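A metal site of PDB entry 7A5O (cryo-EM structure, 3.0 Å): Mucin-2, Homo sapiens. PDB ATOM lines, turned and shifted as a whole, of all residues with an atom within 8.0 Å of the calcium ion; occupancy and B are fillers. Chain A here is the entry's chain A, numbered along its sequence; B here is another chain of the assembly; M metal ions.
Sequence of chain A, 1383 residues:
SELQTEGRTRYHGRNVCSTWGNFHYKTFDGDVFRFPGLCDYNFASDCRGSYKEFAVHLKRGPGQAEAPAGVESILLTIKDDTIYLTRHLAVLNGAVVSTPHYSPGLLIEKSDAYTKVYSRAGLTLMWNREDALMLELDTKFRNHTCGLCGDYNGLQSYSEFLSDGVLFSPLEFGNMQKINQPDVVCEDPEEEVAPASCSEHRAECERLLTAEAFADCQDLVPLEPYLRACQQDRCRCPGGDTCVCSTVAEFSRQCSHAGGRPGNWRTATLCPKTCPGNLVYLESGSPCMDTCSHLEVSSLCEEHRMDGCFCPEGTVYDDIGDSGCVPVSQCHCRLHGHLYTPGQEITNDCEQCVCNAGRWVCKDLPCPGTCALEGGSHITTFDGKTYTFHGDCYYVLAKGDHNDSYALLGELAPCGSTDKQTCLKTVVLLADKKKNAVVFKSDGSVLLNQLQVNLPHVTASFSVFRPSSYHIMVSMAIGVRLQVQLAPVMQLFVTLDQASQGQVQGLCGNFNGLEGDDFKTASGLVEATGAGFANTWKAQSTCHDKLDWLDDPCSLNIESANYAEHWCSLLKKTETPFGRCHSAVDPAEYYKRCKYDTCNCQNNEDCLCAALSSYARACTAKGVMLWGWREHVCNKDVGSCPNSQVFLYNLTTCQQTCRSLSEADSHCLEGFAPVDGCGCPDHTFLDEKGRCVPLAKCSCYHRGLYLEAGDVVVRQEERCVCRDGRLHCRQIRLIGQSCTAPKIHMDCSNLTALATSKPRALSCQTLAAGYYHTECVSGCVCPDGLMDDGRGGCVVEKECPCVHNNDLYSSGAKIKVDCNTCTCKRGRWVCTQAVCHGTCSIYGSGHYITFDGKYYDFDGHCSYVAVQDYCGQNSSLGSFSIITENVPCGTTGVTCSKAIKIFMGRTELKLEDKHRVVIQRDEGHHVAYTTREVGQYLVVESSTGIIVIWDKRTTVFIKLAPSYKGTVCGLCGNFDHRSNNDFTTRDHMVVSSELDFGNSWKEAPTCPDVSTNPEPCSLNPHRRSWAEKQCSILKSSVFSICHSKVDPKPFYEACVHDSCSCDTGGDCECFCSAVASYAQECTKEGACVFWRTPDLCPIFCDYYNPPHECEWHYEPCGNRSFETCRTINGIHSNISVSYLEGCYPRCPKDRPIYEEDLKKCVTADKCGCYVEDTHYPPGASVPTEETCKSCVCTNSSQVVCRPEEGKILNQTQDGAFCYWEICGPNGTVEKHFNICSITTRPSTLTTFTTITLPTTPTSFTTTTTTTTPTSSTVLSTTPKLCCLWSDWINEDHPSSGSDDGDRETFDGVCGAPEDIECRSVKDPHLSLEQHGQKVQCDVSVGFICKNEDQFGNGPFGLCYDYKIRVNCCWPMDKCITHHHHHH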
ATOM      1  N   THR A 850      -8.760   1.156   1.897  1.00  0.00           N
ATOM      2  CA  THR A 850     -10.183   0.939   2.085  1.00  0.00           C
ATOM      3  C   THR A 850     -10.614  -0.344   1.380  1.00  0.00           C
ATOM      4  O   THR A 850      -9.835  -0.993   0.677  1.00  0.00           O
ATOM      5  CB  THR A 850     -10.980   2.138   1.584  1.00  0.00           C
ATOM      6  OG1 THR A 850     -10.819   2.273   0.170  1.00  0.00           O
ATOM      7  CG2 THR A 850     -10.492   3.399   2.240  1.00  0.00           C
ATOM      8  N   PHE A 851     -11.887  -0.731   1.582  1.00  0.00           N
ATOM      9  CA  PHE A 851     -12.453  -1.921   0.940  1.00  0.00           C
ATOM     10  C   PHE A 851     -12.432  -1.833  -0.587  1.00  0.00           C
ATOM     11  O   PHE A 851     -12.474  -2.877  -1.241  1.00  0.00           O
ATOM     12  CB  PHE A 851     -13.907  -2.159   1.359  1.00  0.00           C
ATOM     13  CG  PHE A 851     -14.098  -2.673   2.753  1.00  0.00           C
ATOM     14  CD1 PHE A 851     -13.900  -3.997   3.033  1.00  0.00           C
ATOM     15  CD2 PHE A 851     -14.566  -1.854   3.754  1.00  0.00           C
ATOM     16  CE1 PHE A 851     -14.097  -4.492   4.302  1.00  0.00           C
ATOM     17  CE2 PHE A 851     -14.761  -2.336   5.021  1.00  0.00           C
ATOM     18  CZ  PHE A 851     -14.524  -3.666   5.292  1.00  0.00           C
ATOM     19  N   ASP A 852     -12.406  -0.630  -1.141  1.00  0.00           N
ATOM     20  CA  ASP A 852     -12.350  -0.398  -2.582  1.00  0.00           C
ATOM     21  C   ASP A 852     -10.953  -0.059  -3.055  1.00  0.00           C
ATOM     22  O   ASP A 852     -10.773   0.264  -4.228  1.00  0.00           O
ATOM     23  CB  ASP A 852     -13.321   0.706  -2.961  1.00  0.00           C
ATOM     24  CG  ASP A 852     -14.755   0.286  -2.794  1.00  0.00           C
ATOM     25  OD1 ASP A 852     -15.045  -0.917  -2.934  1.00  0.00           O
ATOM     26  OD2 ASP A 852     -15.599   1.159  -2.522  1.00  0.00           O
ATOM     27  N   GLY A 853      -9.962  -0.101  -2.171  1.00  0.00           N
ATOM     28  CA  GLY A 853      -8.578  -0.001  -2.565  1.00  0.00           C
ATOM     29  C   GLY A 853      -8.044   1.393  -2.720  1.00  0.00           C
ATOM     30  O   GLY A 853      -7.397   1.702  -3.721  1.00  0.00           O
ATOM     31  N   LYS A 854      -8.257   2.246  -1.730  1.00  0.00           N
ATOM     32  CA  LYS A 854      -7.778   3.624  -1.752  1.00  0.00           C
ATOM     33  C   LYS A 854      -6.807   3.823  -0.609  1.00  0.00           C
ATOM     34  O   LYS A 854      -7.160   3.601   0.549  1.00  0.00           O
ATOM     35  CB  LYS A 854      -8.950   4.592  -1.654  1.00  0.00           C
ATOM     36  CG  LYS A 854      -8.598   6.026  -1.810  1.00  0.00           C
ATOM     37  CD  LYS A 854      -9.826   6.863  -1.889  1.00  0.00           C
ATOM     38  CE  LYS A 854      -9.466   8.298  -2.187  1.00  0.00           C
ATOM     39  NZ  LYS A 854     -10.704   9.094  -2.363  1.00  0.00           N
ATOM     40  N   GLY A 966     -22.094  -2.003  -0.036  1.00  0.00           N
ATOM     41  CA  GLY A 966     -22.773  -0.728  -0.024  1.00  0.00           C
ATOM     42  C   GLY A 966     -23.572  -0.456   1.215  1.00  0.00           C
ATOM     43  O   GLY A 966     -24.443   0.424   1.199  1.00  0.00           O
ATOM     44  N   VAL A 968     -21.959  -0.227   4.544  1.00  0.00           N
ATOM     45  CA  VAL A 968     -21.083   0.126   5.653  1.00  0.00           C
ATOM     46  C   VAL A 968     -20.544   1.531   5.429  1.00  0.00           C
ATOM     47  O   VAL A 968     -20.744   2.135   4.378  1.00  0.00           O
ATOM     48  CB  VAL A 968     -19.919  -0.886   5.855  1.00  0.00           C
ATOM     49  CG1 VAL A 968     -20.444  -2.220   6.303  1.00  0.00           C
ATOM     50  CG2 VAL A 968     -19.107  -1.055   4.595  1.00  0.00           C
ATOM     51  N   CYS A 972     -12.957   2.986   6.531  1.00  0.00           N
ATOM     52  CA  CYS A 972     -12.656   1.957   5.558  1.00  0.00           C
ATOM     53  C   CYS A 972     -13.507   2.064   4.301  1.00  0.00           C
ATOM     54  O   CYS A 972     -13.452   1.162   3.467  1.00  0.00           O
ATOM     55  CB  CYS A 972     -12.841   0.567   6.158  1.00  0.00           C
ATOM     56  SG  CYS A 972     -11.654   0.071   7.403  1.00  0.00           S
ATOM     57  N   GLY A 973     -14.315   3.100   4.172  1.00  0.00           N
ATOM     58  CA  GLY A 973     -15.138   3.256   2.991  1.00  0.00           C
ATOM     59  C   GLY A 973     -16.475   2.558   3.117  1.00  0.00           C
ATOM     60  O   GLY A 973     -16.918   2.204   4.216  1.00  0.00           O
ATOM     61  N   ASN A 974     -17.115   2.346   1.969  1.00  0.00           N
ATOM     62  CA  ASN A 974     -18.463   1.800   1.936  1.00  0.00           C
ATOM     63  C   ASN A 974     -18.660   0.545   1.101  1.00  0.00           C
ATOM     64  O   ASN A 974     -19.796   0.070   1.027  1.00  0.00           O
ATOM     65  CB  ASN A 974     -19.469   2.864   1.489  1.00  0.00           C
ATOM     66  CG  ASN A 974     -19.121   3.511   0.172  1.00  0.00           C
ATOM     67  OD1 ASN A 974     -18.171   3.123  -0.492  1.00  0.00           O
ATOM     68  ND2 ASN A 974     -19.893   4.500  -0.203  1.00  0.00           N
ATOM     69  N   PHE A 975     -17.615   0.010   0.463  1.00  0.00           N
ATOM     70  CA  PHE A 975     -17.568  -1.346  -0.117  1.00  0.00           C
ATOM     71  C   PHE A 975     -18.620  -1.521  -1.220  1.00  0.00           C
ATOM     72  O   PHE A 975     -19.459  -2.405  -1.190  1.00  0.00           O
ATOM     73  CB  PHE A 975     -17.664  -2.379   1.018  1.00  0.00           C
ATOM     74  CG  PHE A 975     -17.531  -3.826   0.601  1.00  0.00           C
ATOM     75  CD1 PHE A 975     -16.412  -4.299  -0.033  1.00  0.00           C
ATOM     76  CD2 PHE A 975     -18.471  -4.750   1.021  1.00  0.00           C
ATOM     77  CE1 PHE A 975     -16.302  -5.630  -0.367  1.00  0.00           C
ATOM     78  CE2 PHE A 975     -18.347  -6.088   0.705  1.00  0.00           C
ATOM     79  CZ  PHE A 975     -17.268  -6.521   0.004  1.00  0.00           C
ATOM     80  N   ASP A 976     -18.555  -0.629  -2.208  1.00  0.00           N
ATOM     81  CA  ASP A 976     -19.454  -0.709  -3.353  1.00  0.00           C
ATOM     82  C   ASP A 976     -18.715  -0.712  -4.691  1.00  0.00           C
ATOM     83  O   ASP A 976     -19.311  -0.340  -5.697  1.00  0.00           O
ATOM     84  CB  ASP A 976     -20.492   0.417  -3.335  1.00  0.00           C
ATOM     85  CG  ASP A 976     -19.892   1.801  -3.338  1.00  0.00           C
ATOM     86  OD1 ASP A 976     -18.668   1.944  -3.217  1.00  0.00           O
ATOM     87  OD2 ASP A 976     -20.662   2.759  -3.469  1.00  0.00           O
ATOM     88  N   HIS A 977     -17.440  -1.126  -4.689  1.00  0.00           N
ATOM     89  CA  HIS A 977     -16.632  -1.337  -5.892  1.00  0.00           C
ATOM     90  C   HIS A 977     -16.548  -0.085  -6.760  1.00  0.00           C
ATOM     91  O   HIS A 977     -16.679  -0.149  -7.982  1.00  0.00           O
ATOM     92  CB  HIS A 977     -17.153  -2.527  -6.693  1.00  0.00           C
ATOM     93  CG  HIS A 977     -17.301  -3.769  -5.875  1.00  0.00           C
ATOM     94  ND1 HIS A 977     -16.230  -4.586  -5.558  1.00  0.00           N
ATOM     95  CD2 HIS A 977     -18.383  -4.331  -5.279  1.00  0.00           C
ATOM     96  CE1 HIS A 977     -16.647  -5.592  -4.819  1.00  0.00           C
ATOM     97  NE2 HIS A 977     -17.946  -5.458  -4.633  1.00  0.00           N
ATOM     98  N   ARG A 978     -16.326   1.047  -6.117  1.00  0.00           N
ATOM     99  CA  ARG A 978     -16.296   2.351  -6.771  1.00  0.00           C
ATOM    100  C   ARG A 978     -15.597   3.275  -5.776  1.00  0.00           C
ATOM    101  O   ARG A 978     -16.167   3.574  -4.732  1.00  0.00           O
ATOM    102  CB  ARG A 978     -17.729   2.785  -7.101  1.00  0.00           C
ATOM    103  CG  ARG A 978     -17.964   4.102  -7.782  1.00  0.00           C
ATOM    104  CD  ARG A 978     -18.367   5.092  -6.727  1.00  0.00           C
ATOM    105  NE  ARG A 978     -18.751   6.415  -7.209  1.00  0.00           N
ATOM    106  CZ  ARG A 978     -20.001   6.757  -7.489  1.00  0.00           C
ATOM    107  NH1 ARG A 978     -20.983   5.890  -7.329  1.00  0.00           N
ATOM    108  NH2 ARG A 978     -20.279   7.988  -7.901  1.00  0.00           N
ATOM    109  N   SER A 979     -14.382   3.707  -6.079  1.00  0.00           N
ATOM    110  CA  SER A 979     -13.539   4.270  -5.041  1.00  0.00           C
ATOM    111  C   SER A 979     -13.503   5.784  -5.013  1.00  0.00           C
ATOM    112  O   SER A 979     -12.751   6.341  -4.216  1.00  0.00           O
ATOM    113  CB  SER A 979     -12.103   3.765  -5.167  1.00  0.00           C
ATOM    114  OG  SER A 979     -11.477   4.356  -6.286  1.00  0.00           O
ATOM    115  N   ASN A 980     -14.262   6.477  -5.847  1.00  0.00           N
ATOM    116  CA  ASN A 980     -14.258   7.928  -5.774  1.00  0.00           C
ATOM    117  C   ASN A 980     -15.368   8.470  -4.893  1.00  0.00           C
ATOM    118  O   ASN A 980     -15.764   9.623  -5.045  1.00  0.00           O
ATOM    119  CB  ASN A 980     -14.312   8.556  -7.182  1.00  0.00           C
ATOM    120  CG  ASN A 980     -15.543   8.189  -7.983  1.00  0.00           C
ATOM    121  OD1 ASN A 980     -16.423   7.492  -7.529  1.00  0.00           O
ATOM    122  ND2 ASN A 980     -15.593   8.698  -9.204  1.00  0.00           N
ATOM    123  N   ASN A 981     -15.872   7.654  -3.966  1.00  0.00           N
ATOM    124  CA  ASN A 981     -16.755   8.135  -2.925  1.00  0.00           C
ATOM    125  C   ASN A 981     -16.395   7.581  -1.553  1.00  0.00           C
ATOM    126  O   ASN A 981     -17.220   7.631  -0.645  1.00  0.00           O
ATOM    127  CB  ASN A 981     -18.227   7.845  -3.268  1.00  0.00           C
ATOM    128  CG  ASN A 981     -18.526   6.375  -3.467  1.00  0.00           C
ATOM    129  OD1 ASN A 981     -17.684   5.509  -3.320  1.00  0.00           O
ATOM    130  ND2 ASN A 981     -19.772   6.091  -3.788  1.00  0.00           N
ATOM    131  N   ASP A 982     -15.188   7.047  -1.396  1.00  0.00           N
ATOM    132  CA  ASP A 982     -14.773   6.540  -0.095  1.00  0.00           C
ATOM    133  C   ASP A 982     -14.529   7.641   0.920  1.00  0.00           C
ATOM    134  O   ASP A 982     -14.536   7.362   2.125  1.00  0.00           O
ATOM    135  CB  ASP A 982     -13.521   5.682  -0.203  1.00  0.00           C
ATOM    136  CG  ASP A 982     -13.788   4.340  -0.791  1.00  0.00           C
ATOM    137  OD1 ASP A 982     -14.926   3.854  -0.694  1.00  0.00           O
ATOM    138  OD2 ASP A 982     -12.839   3.723  -1.292  1.00  0.00           O
ATOM    139  N   PHE A 983     -14.301   8.875   0.486  1.00  0.00           N
ATOM    140  CA  PHE A 983     -14.178   9.983   1.429  1.00  0.00           C
ATOM    141  C   PHE A 983     -15.523  10.644   1.684  1.00  0.00           C
ATOM    142  O   PHE A 983     -15.675  11.852   1.550  1.00  0.00           O
ATOM    143  CB  PHE A 983     -13.148  10.997   0.969  1.00  0.00           C
ATOM    144  CG  PHE A 983     -11.718  10.535   1.046  1.00  0.00           C
ATOM    145  CD1 PHE A 983     -11.385   9.327   1.625  1.00  0.00           C
ATOM    146  CD2 PHE A 983     -10.701  11.362   0.631  1.00  0.00           C
ATOM    147  CE1 PHE A 983     -10.085   8.922   1.723  1.00  0.00           C
ATOM    148  CE2 PHE A 983      -9.389  10.957   0.740  1.00  0.00           C
ATOM    149  CZ  PHE A 983      -9.085   9.749   1.282  1.00  0.00           C
ATOM    150  N   THR A 984     -16.509   9.852   2.073  1.00  0.00           N
ATOM    151  CA  THR A 984     -17.789  10.354   2.540  1.00  0.00           C
ATOM    152  C   THR A 984     -17.697  10.564   4.052  1.00  0.00           C
ATOM    153  O   THR A 984     -17.284   9.661   4.777  1.00  0.00           O
ATOM    154  CB  THR A 984     -18.916   9.376   2.228  1.00  0.00           C
ATOM    155  OG1 THR A 984     -18.982   9.169   0.820  1.00  0.00           O
ATOM    156  CG2 THR A 984     -20.233   9.937   2.670  1.00  0.00           C
ATOM    157  N   GLY B 513     -14.933   5.286 -12.373  1.00  0.00           N
ATOM    158  CA  GLY B 513     -15.040   5.667 -10.988  1.00  0.00           C
ATOM    159  C   GLY B 513     -14.077   4.949 -10.066  1.00  0.00           C
ATOM    160  O   GLY B 513     -13.581   5.564  -9.119  1.00  0.00           O
ATOM    161  N   LEU B 514     -13.816   3.682 -10.300  1.00  0.00           N
ATOM    162  CA  LEU B 514     -12.832   2.909  -9.553  1.00  0.00           C
ATOM    163  C   LEU B 514     -11.463   3.046 -10.211  1.00  0.00           C
ATOM    164  O   LEU B 514     -11.363   3.107 -11.433  1.00  0.00           O
ATOM    165  CB  LEU B 514     -13.246   1.428  -9.531  1.00  0.00           C
ATOM    166  CG  LEU B 514     -12.430   0.355  -8.828  1.00  0.00           C
ATOM    167  CD1 LEU B 514     -12.402   0.529  -7.339  1.00  0.00           C
ATOM    168  CD2 LEU B 514     -13.008  -0.989  -9.194  1.00  0.00           C
HETATM  169 CA    CA M   1     -16.641   3.140  -2.369  1.00  0.00          CA
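The calcium ion is bound by the side-chain carboxylate of Asp 852, the side-chain amide oxygen of Asn 974, the backbone carbonyl oxygen of Arg 978, the side-chain carboxylate of Asp 982, the side-chain carboxylate of Asp 976 and the side-chain amide oxygen of Asn 981. The calcium ion has six donor atoms within binding distance.
Of the 22 residues printed, 6 come within 4 Å of the calcium ion.
The backbone carbonyl oxygen of Asn 974 sits close to the backbone NH of Gly 966. The side-chain carboxylate (OD2) of Asp 982 lies within hydrogen-bond range of the side-chain hydroxyl (OG1) of Thr 850, 2.9 Å away. The guanidinium group (NE) of Arg 978 lies within hydrogen-bond range of the side-chain amide oxygen (OD1) of Asn 980. OG1 of Thr 984 is in hydrogen-bond range of O of Asn 981, 2.8 Å away. OD1 of Asp 852 is in hydrogen-bond range of N of His 977 (3.0 Å).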
